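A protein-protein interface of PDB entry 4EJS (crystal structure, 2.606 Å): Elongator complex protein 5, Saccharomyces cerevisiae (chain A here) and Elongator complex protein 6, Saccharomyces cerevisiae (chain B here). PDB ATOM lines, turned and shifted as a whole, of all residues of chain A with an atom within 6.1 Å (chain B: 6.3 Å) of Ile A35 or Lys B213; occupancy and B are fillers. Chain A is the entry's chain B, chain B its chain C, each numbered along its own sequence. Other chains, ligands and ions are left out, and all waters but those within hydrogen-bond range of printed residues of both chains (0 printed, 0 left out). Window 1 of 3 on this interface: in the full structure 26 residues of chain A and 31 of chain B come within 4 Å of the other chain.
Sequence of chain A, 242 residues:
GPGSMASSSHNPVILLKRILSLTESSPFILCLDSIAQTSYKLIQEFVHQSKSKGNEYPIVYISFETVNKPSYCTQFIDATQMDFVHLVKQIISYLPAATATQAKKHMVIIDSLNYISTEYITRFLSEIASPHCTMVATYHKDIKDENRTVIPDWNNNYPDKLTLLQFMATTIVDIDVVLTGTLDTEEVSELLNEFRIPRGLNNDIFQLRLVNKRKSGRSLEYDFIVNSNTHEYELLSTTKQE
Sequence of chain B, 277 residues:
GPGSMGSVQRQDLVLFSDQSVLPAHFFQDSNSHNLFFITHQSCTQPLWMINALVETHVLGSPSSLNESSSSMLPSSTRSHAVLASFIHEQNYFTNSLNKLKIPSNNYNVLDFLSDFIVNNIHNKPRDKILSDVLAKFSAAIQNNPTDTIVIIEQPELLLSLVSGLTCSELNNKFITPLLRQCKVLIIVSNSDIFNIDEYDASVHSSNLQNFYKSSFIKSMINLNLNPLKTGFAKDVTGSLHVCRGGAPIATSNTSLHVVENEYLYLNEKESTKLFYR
OD2 of Asp A142 sits at hydrogen-bond distance from N of Ile A35, at 3.1 Å. The backbone carbonyl oxygen (O) of Ile A35 lies close to the side-chain amide oxygen (OD1) of Asn A202, at 3.0 Å. The backbone carbonyl oxygen (O) of Ala A36 is in hydrogen-bond range of the backbone NH (N) of Asn A202, 3.0 Å away. N of Thr A38 sits close to ND2 of Asn A202, at 3.1 Å. The side-chain amino group of Lys B218 lies within hydrogen-bond range of the side-chain hydroxyl of Ser B214, 3.5 Å away. The backbone carbonyl oxygen (O) of Phe B216 sits at hydrogen-bond distance from the backbone NH (N) of Gly B246 (3.0 Å).
Among the printed residues, pairs that only touch across the chains: Ile A35 with Lys B213 (3.5 Å), Ile A35 with Phe B216 (3.4 Å), Ile A35 with Ile B217 (3.2 Å), Ile A143 with Asn B210 (3.7 Å), Ile A143 with Lys B213 (3.3 Å), Ile A143 with Ser B214 (3.95 Å), Lys A144 with Gln B209 (3.6 Å), Asn A193 with Phe B194 (3.6 Å), Glu A194 with Phe B194 (3.3 Å), Phe A195 with Phe B37 (3.6 Å), Phe A195 with Phe B194 (3.8 Å), Phe A195 with Tyr B212 (3.6 Å), Ile A197 with Phe B216 (3.9 Å) and Asn A202 with Phe B216 (3.9 Å).
Of the 15 printed residues of chain B, 11 touch a printed residue of chain A. Hydrophobic or aromatic side chains of chain B that line the printed part of chain A: Phe B37, Phe B194, Phe B216 and Ile B217. Of the 16 printed residues of chain A, 10 touch a printed residue of chain B. Hydrophobic or aromatic side chains of chain A that line the printed part of chain B: Ile A35, Ile A143, Phe A195 and Ile A197. Along chain A the printed residues that touch a printed residue of chain B span positions 35 to 202. Among the printed residues, 18 pairs touch across the chains.
The side-chain hydroxyl of Thr A38 is in hydrogen-bond range of the backbone carbonyl oxygen of Gly B246, at 2.7 Å. The backbone carbonyl oxygen (O) of Lys A144 sits at hydrogen-bond distance from the side-chain amide nitrogen (ND2) of Asn B210 (2.8 Å). O of Leu A192 sits at hydrogen-bond distance from NZ of Lys B213 (3.1 Å). O of Gly B245 sits close to OD1 of Asn A202.
Ile A35 touches three residues of chain B. Of the printed residues of chain B, Thr A38 touches Gly B246. Printed residues of chain A within 4 Å of Phe B194: Asn A193, Glu A194 and Phe A195. Printed residues of chain A within 4 Å of Ser B214: Ile A143. Of the printed residues of chain A, Phe B216 touches Ile A35, Ile A197 and Asn A202. Of the printed residues of chain A, Gly B245 touches Asn A202 (3.5 Å).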
ATOM      1  N   ASP A  33      23.169  13.792  17.646  1.00  0.00           N
ATOM      2  CA  ASP A  33      23.779  14.952  18.272  1.00  0.00           C
ATOM      3  C   ASP A  33      23.021  16.243  17.983  1.00  0.00           C
ATOM      4  O   ASP A  33      21.970  16.233  17.344  1.00  0.00           O
ATOM      5  CB  ASP A  33      25.248  15.071  17.864  1.00  0.00           C
ATOM      6  CG  ASP A  33      25.422  15.604  16.468  1.00  0.00           C
ATOM      7  OD1 ASP A  33      26.563  15.961  16.102  1.00  0.00           O
ATOM      8  OD2 ASP A  33      24.418  15.665  15.735  1.00  0.00           O
ATOM      9  N   SER A  34      23.563  17.350  18.472  1.00  0.00           N
ATOM     10  CA  SER A  34      22.981  18.666  18.239  1.00  0.00           C
ATOM     11  C   SER A  34      24.046  19.741  18.410  1.00  0.00           C
ATOM     12  O   SER A  34      25.192  19.460  18.779  1.00  0.00           O
ATOM     13  CB  SER A  34      21.793  18.929  19.186  1.00  0.00           C
ATOM     14  OG  SER A  34      22.197  19.030  20.547  1.00  0.00           O
ATOM     15  N   ILE A  35      23.654  20.971  18.124  1.00  0.00           N
ATOM     16  CA  ILE A  35      24.490  22.150  18.299  1.00  0.00           C
ATOM     17  C   ILE A  35      25.068  22.227  19.718  1.00  0.00           C
ATOM     18  O   ILE A  35      26.156  22.768  19.926  1.00  0.00           O
ATOM     19  CB  ILE A  35      23.639  23.414  17.997  1.00  0.00           C
ATOM     20  CG1 ILE A  35      23.849  23.836  16.559  1.00  0.00           C
ATOM     21  CG2 ILE A  35      23.968  24.558  18.922  1.00  0.00           C
ATOM     22  CD1 ILE A  35      24.034  22.676  15.659  1.00  0.00           C
ATOM     23  N   ALA A  36      24.336  21.689  20.693  1.00  0.00           N
ATOM     24  CA  ALA A  36      24.734  21.809  22.087  1.00  0.00           C
ATOM     25  C   ALA A  36      25.922  20.916  22.420  1.00  0.00           C
ATOM     26  O   ALA A  36      26.673  21.185  23.352  1.00  0.00           O
ATOM     27  CB  ALA A  36      23.564  21.488  22.998  1.00  0.00           C
ATOM     28  N   GLN A  37      26.085  19.853  21.651  1.00  0.00           N
ATOM     29  CA  GLN A  37      27.143  18.885  21.894  1.00  0.00           C
ATOM     30  C   GLN A  37      27.281  18.004  20.667  1.00  0.00           C
ATOM     31  O   GLN A  37      26.562  17.023  20.515  1.00  0.00           O
ATOM     32  CB  GLN A  37      26.794  18.009  23.089  1.00  0.00           C
ATOM     33  CG  GLN A  37      27.919  17.062  23.483  1.00  0.00           C
ATOM     34  CD  GLN A  37      29.083  17.790  24.115  1.00  0.00           C
ATOM     35  OE1 GLN A  37      28.885  18.691  24.914  1.00  0.00           O
ATOM     36  NE2 GLN A  37      30.303  17.417  23.747  1.00  0.00           N
ATOM     37  N   THR A  38      28.186  18.366  19.773  1.00  0.00           N
ATOM     38  CA  THR A  38      28.370  17.583  18.561  1.00  0.00           C
ATOM     39  C   THR A  38      29.012  16.226  18.877  1.00  0.00           C
ATOM     40  O   THR A  38      29.338  15.937  20.025  1.00  0.00           O
ATOM     41  CB  THR A  38      29.159  18.361  17.517  1.00  0.00           C
ATOM     42  OG1 THR A  38      30.498  18.570  17.987  1.00  0.00           O
ATOM     43  CG2 THR A  38      28.494  19.707  17.285  1.00  0.00           C
ATOM     44  N   ASP A 142      18.957  18.561  15.172  1.00  0.00           N
ATOM     45  CA  ASP A 142      18.350  19.860  14.913  1.00  0.00           C
ATOM     46  C   ASP A 142      18.450  20.410  13.479  1.00  0.00           C
ATOM     47  O   ASP A 142      18.012  21.542  13.223  1.00  0.00           O
ATOM     48  CB  ASP A 142      18.808  20.900  15.947  1.00  0.00           C
ATOM     49  CG  ASP A 142      20.315  20.878  16.192  1.00  0.00           C
ATOM     50  OD1 ASP A 142      21.031  20.176  15.443  1.00  0.00           O
ATOM     51  OD2 ASP A 142      20.777  21.576  17.133  1.00  0.00           O
ATOM     52  N   ILE A 143      19.013  19.622  12.554  1.00  0.00           N
ATOM     53  CA  ILE A 143      18.925  19.916  11.115  1.00  0.00           C
ATOM     54  C   ILE A 143      17.672  19.237  10.529  1.00  0.00           C
ATOM     55  O   ILE A 143      17.524  18.022  10.607  1.00  0.00           O
ATOM     56  CB  ILE A 143      20.173  19.443  10.334  1.00  0.00           C
ATOM     57  CG1 ILE A 143      21.437  20.087  10.883  1.00  0.00           C
ATOM     58  CG2 ILE A 143      20.056  19.774   8.850  1.00  0.00           C
ATOM     59  CD1 ILE A 143      21.367  21.547  10.904  1.00  0.00           C
ATOM     60  N   LYS A 144      16.771  20.029   9.958  1.00  0.00           N
ATOM     61  CA  LYS A 144      15.445  19.549   9.548  1.00  0.00           C
ATOM     62  C   LYS A 144      15.491  19.043   8.112  1.00  0.00           C
ATOM     63  O   LYS A 144      16.349  19.465   7.347  1.00  0.00           O
ATOM     64  CB  LYS A 144      14.420  20.678   9.716  1.00  0.00           C
ATOM     65  CG  LYS A 144      14.548  21.436  11.063  1.00  0.00           C
ATOM     66  CD  LYS A 144      14.359  22.960  10.876  1.00  0.00           C
ATOM     67  CE  LYS A 144      15.036  23.819  11.980  1.00  0.00           C
ATOM     68  NZ  LYS A 144      16.466  24.234  11.710  1.00  0.00           N
ATOM     69  N   LEU A 192      18.372  27.431  21.833  1.00  0.00           N
ATOM     70  CA  LEU A 192      18.968  27.091  20.545  1.00  0.00           C
ATOM     71  C   LEU A 192      17.941  27.181  19.422  1.00  0.00           C
ATOM     72  O   LEU A 192      18.272  27.546  18.302  1.00  0.00           O
ATOM     73  CB  LEU A 192      19.627  25.712  20.578  1.00  0.00           C
ATOM     74  CG  LEU A 192      20.704  25.596  21.653  1.00  0.00           C
ATOM     75  CD1 LEU A 192      21.272  24.212  21.667  1.00  0.00           C
ATOM     76  CD2 LEU A 192      21.787  26.629  21.425  1.00  0.00           C
ATOM     77  N   ASN A 193      16.685  26.882  19.728  1.00  0.00           N
ATOM     78  CA  ASN A 193      15.646  27.024  18.716  1.00  0.00           C
ATOM     79  C   ASN A 193      15.609  28.440  18.121  1.00  0.00           C
ATOM     80  O   ASN A 193      15.239  28.628  16.958  1.00  0.00           O
ATOM     81  CB  ASN A 193      14.273  26.614  19.262  1.00  0.00           C
ATOM     82  CG  ASN A 193      13.258  26.369  18.153  1.00  0.00           C
ATOM     83  OD1 ASN A 193      13.359  25.383  17.412  1.00  0.00           O
ATOM     84  ND2 ASN A 193      12.281  27.272  18.025  1.00  0.00           N
ATOM     85  N   GLU A 194      16.001  29.431  18.912  1.00  0.00           N
ATOM     86  CA  GLU A 194      16.032  30.806  18.437  1.00  0.00           C
ATOM     87  C   GLU A 194      17.452  31.265  18.103  1.00  0.00           C
ATOM     88  O   GLU A 194      17.712  32.477  17.999  1.00  0.00           O
ATOM     89  CB  GLU A 194      15.427  31.740  19.481  1.00  0.00           C
ATOM     90  CG  GLU A 194      14.030  31.357  19.932  1.00  0.00           C
ATOM     91  CD  GLU A 194      13.529  32.239  21.064  1.00  0.00           C
ATOM     92  OE1 GLU A 194      13.334  33.455  20.841  1.00  0.00           O
ATOM     93  OE2 GLU A 194      13.347  31.715  22.184  1.00  0.00           O
ATOM     94  N   PHE A 195      18.356  30.297  17.942  1.00  0.00           N
ATOM     95  CA  PHE A 195      19.793  30.567  17.773  1.00  0.00           C
ATOM     96  C   PHE A 195      20.345  31.585  18.785  1.00  0.00           C
ATOM     97  O   PHE A 195      21.042  32.531  18.422  1.00  0.00           O
ATOM     98  CB  PHE A 195      20.152  30.998  16.333  1.00  0.00           C
ATOM     99  CG  PHE A 195      21.558  30.631  15.944  1.00  0.00           C
ATOM    100  CD1 PHE A 195      21.855  29.341  15.505  1.00  0.00           C
ATOM    101  CD2 PHE A 195      22.594  31.550  16.069  1.00  0.00           C
ATOM    102  CE1 PHE A 195      23.154  28.970  15.190  1.00  0.00           C
ATOM    103  CE2 PHE A 195      23.900  31.187  15.754  1.00  0.00           C
ATOM    104  CZ  PHE A 195      24.180  29.898  15.316  1.00  0.00           C
ATOM    105  N   ILE A 197      22.875  31.318  21.584  1.00  0.00           N
ATOM    106  CA  ILE A 197      23.881  30.372  22.025  1.00  0.00           C
ATOM    107  C   ILE A 197      24.405  30.828  23.369  1.00  0.00           C
ATOM    108  O   ILE A 197      24.988  31.904  23.475  1.00  0.00           O
ATOM    109  CB  ILE A 197      25.047  30.301  21.033  1.00  0.00           C
ATOM    110  CG1 ILE A 197      24.494  30.232  19.607  1.00  0.00           C
ATOM    111  CG2 ILE A 197      25.984  29.126  21.376  1.00  0.00           C
ATOM    112  CD1 ILE A 197      23.650  28.992  19.346  1.00  0.00           C
ATOM    113  N   LEU A 201      28.523  25.237  26.290  1.00  0.00           N
ATOM    114  CA  LEU A 201      28.169  24.065  25.484  1.00  0.00           C
ATOM    115  C   LEU A 201      29.435  23.423  24.920  1.00  0.00           C
ATOM    116  O   LEU A 201      30.527  23.984  25.036  1.00  0.00           O
ATOM    117  CB  LEU A 201      27.214  24.418  24.345  1.00  0.00           C
ATOM    118  CG  LEU A 201      25.982  25.267  24.659  1.00  0.00           C
ATOM    119  CD1 LEU A 201      25.231  25.547  23.375  1.00  0.00           C
ATOM    120  CD2 LEU A 201      25.082  24.594  25.671  1.00  0.00           C
ATOM    121  N   ASN A 202      29.287  22.245  24.320  1.00  0.00           N
ATOM    122  CA  ASN A 202      30.405  21.565  23.646  1.00  0.00           C
ATOM    123  C   ASN A 202      31.649  21.335  24.500  1.00  0.00           C
ATOM    124  O   ASN A 202      32.738  21.838  24.208  1.00  0.00           O
ATOM    125  CB  ASN A 202      30.771  22.289  22.357  1.00  0.00           C
ATOM    126  CG  ASN A 202      29.723  22.103  21.274  1.00  0.00           C
ATOM    127  OD1 ASN A 202      28.967  23.028  20.965  1.00  0.00           O
ATOM    128  ND2 ASN A 202      29.677  20.903  20.686  1.00  0.00           N
ATOM    129  N   PHE B  37      32.125  31.497  12.506  1.00  0.00           N
ATOM    130  CA  PHE B  37      30.761  31.829  12.155  1.00  0.00           C
ATOM    131  C   PHE B  37      30.280  33.035  12.982  1.00  0.00           C
ATOM    132  O   PHE B  37      30.210  32.988  14.207  1.00  0.00           O
ATOM    133  CB  PHE B  37      29.858  30.618  12.345  1.00  0.00           C
ATOM    134  CG  PHE B  37      28.443  30.838  11.899  1.00  0.00           C
ATOM    135  CD1 PHE B  37      28.171  31.416  10.665  1.00  0.00           C
ATOM    136  CD2 PHE B  37      27.381  30.448  12.706  1.00  0.00           C
ATOM    137  CE1 PHE B  37      26.864  31.598  10.235  1.00  0.00           C
ATOM    138  CE2 PHE B  37      26.073  30.617  12.286  1.00  0.00           C
ATOM    139  CZ  PHE B  37      25.814  31.199  11.040  1.00  0.00           C
ATOM    140  N   PHE B 194      15.451  34.262  13.025  1.00  0.00           N
ATOM    141  CA  PHE B 194      15.219  33.606  14.314  1.00  0.00           C
ATOM    142  C   PHE B 194      14.520  34.528  15.296  1.00  0.00           C
ATOM    143  O   PHE B 194      14.155  34.114  16.387  1.00  0.00           O
ATOM    144  CB  PHE B 194      16.549  33.162  14.939  1.00  0.00           C
ATOM    145  CG  PHE B 194      17.204  32.022  14.222  1.00  0.00           C
ATOM    146  CD1 PHE B 194      16.825  30.711  14.486  1.00  0.00           C
ATOM    147  CD2 PHE B 194      18.205  32.254  13.287  1.00  0.00           C
ATOM    148  CE1 PHE B 194      17.428  29.654  13.831  1.00  0.00           C
ATOM    149  CE2 PHE B 194      18.799  31.199  12.619  1.00  0.00           C
ATOM    150  CZ  PHE B 194      18.418  29.897  12.898  1.00  0.00           C
ATOM    151  N   LEU B 208      16.488  27.753   5.543  1.00  0.00           N
ATOM    152  CA  LEU B 208      17.335  28.862   5.910  1.00  0.00           C
ATOM    153  C   LEU B 208      18.001  28.667   7.280  1.00  0.00           C
ATOM    154  O   LEU B 208      19.192  28.923   7.445  1.00  0.00           O
ATOM    155  CB  LEU B 208      16.475  30.111   5.950  1.00  0.00           C
ATOM    156  CG  LEU B 208      16.997  31.312   5.192  1.00  0.00           C
ATOM    157  CD1 LEU B 208      15.948  32.403   5.249  1.00  0.00           C
ATOM    158  CD2 LEU B 208      18.335  31.757   5.790  1.00  0.00           C
ATOM    159  N   GLN B 209      17.217  28.225   8.259  1.00  0.00           N
ATOM    160  CA  GLN B 209      17.706  27.985   9.616  1.00  0.00           C
ATOM    161  C   GLN B 209      18.737  26.878   9.680  1.00  0.00           C
ATOM    162  O   GLN B 209      19.659  26.945  10.485  1.00  0.00           O
ATOM    163  CB  GLN B 209      16.545  27.671  10.562  1.00  0.00           C
ATOM    164  CG  GLN B 209      15.690  28.916  10.902  1.00  0.00           C
ATOM    165  CD  GLN B 209      14.607  28.663  11.954  1.00  0.00           C
ATOM    166  OE1 GLN B 209      14.465  27.552  12.477  1.00  0.00           O
ATOM    167  NE2 GLN B 209      13.838  29.702  12.263  1.00  0.00           N
ATOM    168  N   ASN B 210      18.580  25.863   8.832  1.00  0.00           N
ATOM    169  CA  ASN B 210      19.550  24.767   8.737  1.00  0.00           C
ATOM    170  C   ASN B 210      20.939  25.285   8.417  1.00  0.00           C
ATOM    171  O   ASN B 210      21.932  24.722   8.852  1.00  0.00           O
ATOM    172  CB  ASN B 210      19.140  23.737   7.674  1.00  0.00           C
ATOM    173  CG  ASN B 210      18.037  22.819   8.146  1.00  0.00           C
ATOM    174  OD1 ASN B 210      17.638  22.850   9.311  1.00  0.00           O
ATOM    175  ND2 ASN B 210      17.543  21.989   7.248  1.00  0.00           N
ATOM    176  N   PHE B 211      20.998  26.368   7.655  1.00  0.00           N
ATOM    177  CA  PHE B 211      22.276  26.946   7.276  1.00  0.00           C
ATOM    178  C   PHE B 211      23.043  27.487   8.495  1.00  0.00           C
ATOM    179  O   PHE B 211      24.257  27.354   8.582  1.00  0.00           O
ATOM    180  CB  PHE B 211      22.082  28.034   6.216  1.00  0.00           C
ATOM    181  CG  PHE B 211      23.359  28.711   5.826  1.00  0.00           C
ATOM    182  CD1 PHE B 211      24.156  28.189   4.807  1.00  0.00           C
ATOM    183  CD2 PHE B 211      23.786  29.845   6.499  1.00  0.00           C
ATOM    184  CE1 PHE B 211      25.336  28.797   4.452  1.00  0.00           C
ATOM    185  CE2 PHE B 211      24.980  30.458   6.158  1.00  0.00           C
ATOM    186  CZ  PHE B 211      25.758  29.935   5.130  1.00  0.00           C
ATOM    187  N   TYR B 212      22.323  28.084   9.433  1.00  0.00           N
ATOM    188  CA  TYR B 212      22.916  28.568  10.679  1.00  0.00           C
ATOM    189  C   TYR B 212      23.368  27.435  11.592  1.00  0.00           C
ATOM    190  O   TYR B 212      24.443  27.509  12.178  1.00  0.00           O
ATOM    191  CB  TYR B 212      21.958  29.515  11.407  1.00  0.00           C
ATOM    192  CG  TYR B 212      21.600  30.733  10.583  1.00  0.00           C
ATOM    193  CD1 TYR B 212      22.135  31.992  10.872  1.00  0.00           C
ATOM    194  CD2 TYR B 212      20.737  30.621   9.505  1.00  0.00           C
ATOM    195  CE1 TYR B 212      21.803  33.111  10.091  1.00  0.00           C
ATOM    196  CE2 TYR B 212      20.409  31.721   8.723  1.00  0.00           C
ATOM    197  CZ  TYR B 212      20.944  32.954   9.011  1.00  0.00           C
ATOM    198  OH  TYR B 212      20.586  34.018   8.220  1.00  0.00           O
ATOM    199  N   LYS B 213      22.562  26.382  11.704  1.00  0.00           N
ATOM    200  CA  LYS B 213      22.918  25.228  12.528  1.00  0.00           C
ATOM    201  C   LYS B 213      24.101  24.505  11.901  1.00  0.00           C
ATOM    202  O   LYS B 213      25.019  24.072  12.579  1.00  0.00           O
ATOM    203  CB  LYS B 213      21.734  24.276  12.649  1.00  0.00           C
ATOM    204  CG  LYS B 213      20.421  24.939  13.043  1.00  0.00           C
ATOM    205  CD  LYS B 213      20.376  25.253  14.519  1.00  0.00           C
ATOM    206  CE  LYS B 213      19.047  25.905  14.895  1.00  0.00           C
ATOM    207  NZ  LYS B 213      18.426  25.294  16.115  1.00  0.00           N
ATOM    208  N   SER B 214      24.076  24.408  10.585  1.00  0.00           N
ATOM    209  CA  SER B 214      25.133  23.778   9.822  1.00  0.00           C
ATOM    210  C   SER B 214      26.464  24.526   9.939  1.00  0.00           C
ATOM    211  O   SER B 214      27.527  23.917  10.092  1.00  0.00           O
ATOM    212  CB  SER B 214      24.704  23.710   8.355  1.00  0.00           C
ATOM    213  OG  SER B 214      25.576  22.904   7.613  1.00  0.00           O
ATOM    214  N   SER B 215      26.410  25.849   9.844  1.00  0.00           N
ATOM    215  CA  SER B 215      27.627  26.657   9.870  1.00  0.00           C
ATOM    216  C   SER B 215      28.240  26.601  11.256  1.00  0.00           C
ATOM    217  O   SER B 215      29.457  26.521  11.392  1.00  0.00           O
ATOM    218  CB  SER B 215      27.337  28.111   9.474  1.00  0.00           C
ATOM    219  OG  SER B 215      26.735  28.195   8.197  1.00  0.00           O
ATOM    220  N   PHE B 216      27.383  26.633  12.277  1.00  0.00           N
ATOM    221  CA  PHE B 216      27.821  26.519  13.668  1.00  0.00           C
ATOM    222  C   PHE B 216      28.519  25.189  13.956  1.00  0.00           C
ATOM    223  O   PHE B 216      29.574  25.157  14.583  1.00  0.00           O
ATOM    224  CB  PHE B 216      26.650  26.701  14.627  1.00  0.00           C
ATOM    225  CG  PHE B 216      27.034  26.565  16.065  1.00  0.00           C
ATOM    226  CD1 PHE B 216      27.177  25.311  16.644  1.00  0.00           C
ATOM    227  CD2 PHE B 216      27.268  27.689  16.842  1.00  0.00           C
ATOM    228  CE1 PHE B 216      27.554  25.182  17.979  1.00  0.00           C
ATOM    229  CE2 PHE B 216      27.635  27.564  18.166  1.00  0.00           C
ATOM    230  CZ  PHE B 216      27.784  26.301  18.729  1.00  0.00           C
ATOM    231  N   ILE B 217      27.914  24.101  13.497  1.00  0.00           N
ATOM    232  CA  ILE B 217      28.498  22.767  13.590  1.00  0.00           C
ATOM    233  C   ILE B 217      29.886  22.666  12.953  1.00  0.00           C
ATOM    234  O   ILE B 217      30.754  21.945  13.448  1.00  0.00           O
ATOM    235  CB  ILE B 217      27.570  21.746  12.925  1.00  0.00           C
ATOM    236  CG1 ILE B 217      26.405  21.416  13.856  1.00  0.00           C
ATOM    237  CG2 ILE B 217      28.323  20.483  12.550  1.00  0.00           C
ATOM    238  CD1 ILE B 217      25.254  20.743  13.141  1.00  0.00           C
ATOM    239  N   LYS B 218      30.089  23.367  11.842  1.00  0.00           N
ATOM    240  CA  LYS B 218      31.370  23.328  11.138  1.00  0.00           C
ATOM    241  C   LYS B 218      32.362  24.344  11.724  1.00  0.00           C
ATOM    242  O   LYS B 218      33.572  24.258  11.490  1.00  0.00           O
ATOM    243  CB  LYS B 218      31.164  23.607   9.644  1.00  0.00           C
ATOM    244  CG  LYS B 218      30.841  22.387   8.821  1.00  0.00           C
ATOM    245  CD  LYS B 218      29.628  22.610   7.958  1.00  0.00           C
ATOM    246  CE  LYS B 218      29.895  23.584   6.837  1.00  0.00           C
ATOM    247  NZ  LYS B 218      28.594  24.255   6.505  1.00  0.00           N
ATOM    248  N   GLY B 245      32.372  26.803  18.807  1.00  0.00           N
ATOM    249  CA  GLY B 245      31.586  26.225  17.731  1.00  0.00           C
ATOM    250  C   GLY B 245      31.390  24.743  17.986  1.00  0.00           C
ATOM    251  O   GLY B 245      31.606  24.251  19.096  1.00  0.00           O
ATOM    252  N   GLY B 246      30.994  24.016  16.950  1.00  0.00           N
ATOM    253  CA  GLY B 246      30.743  22.602  17.093  1.00  0.00           C
ATOM    254  C   GLY B 246      31.931  21.773  16.661  1.00  0.00           C
ATOM    255  O   GLY B 246      31.970  20.573  16.937  1.00  0.00           O
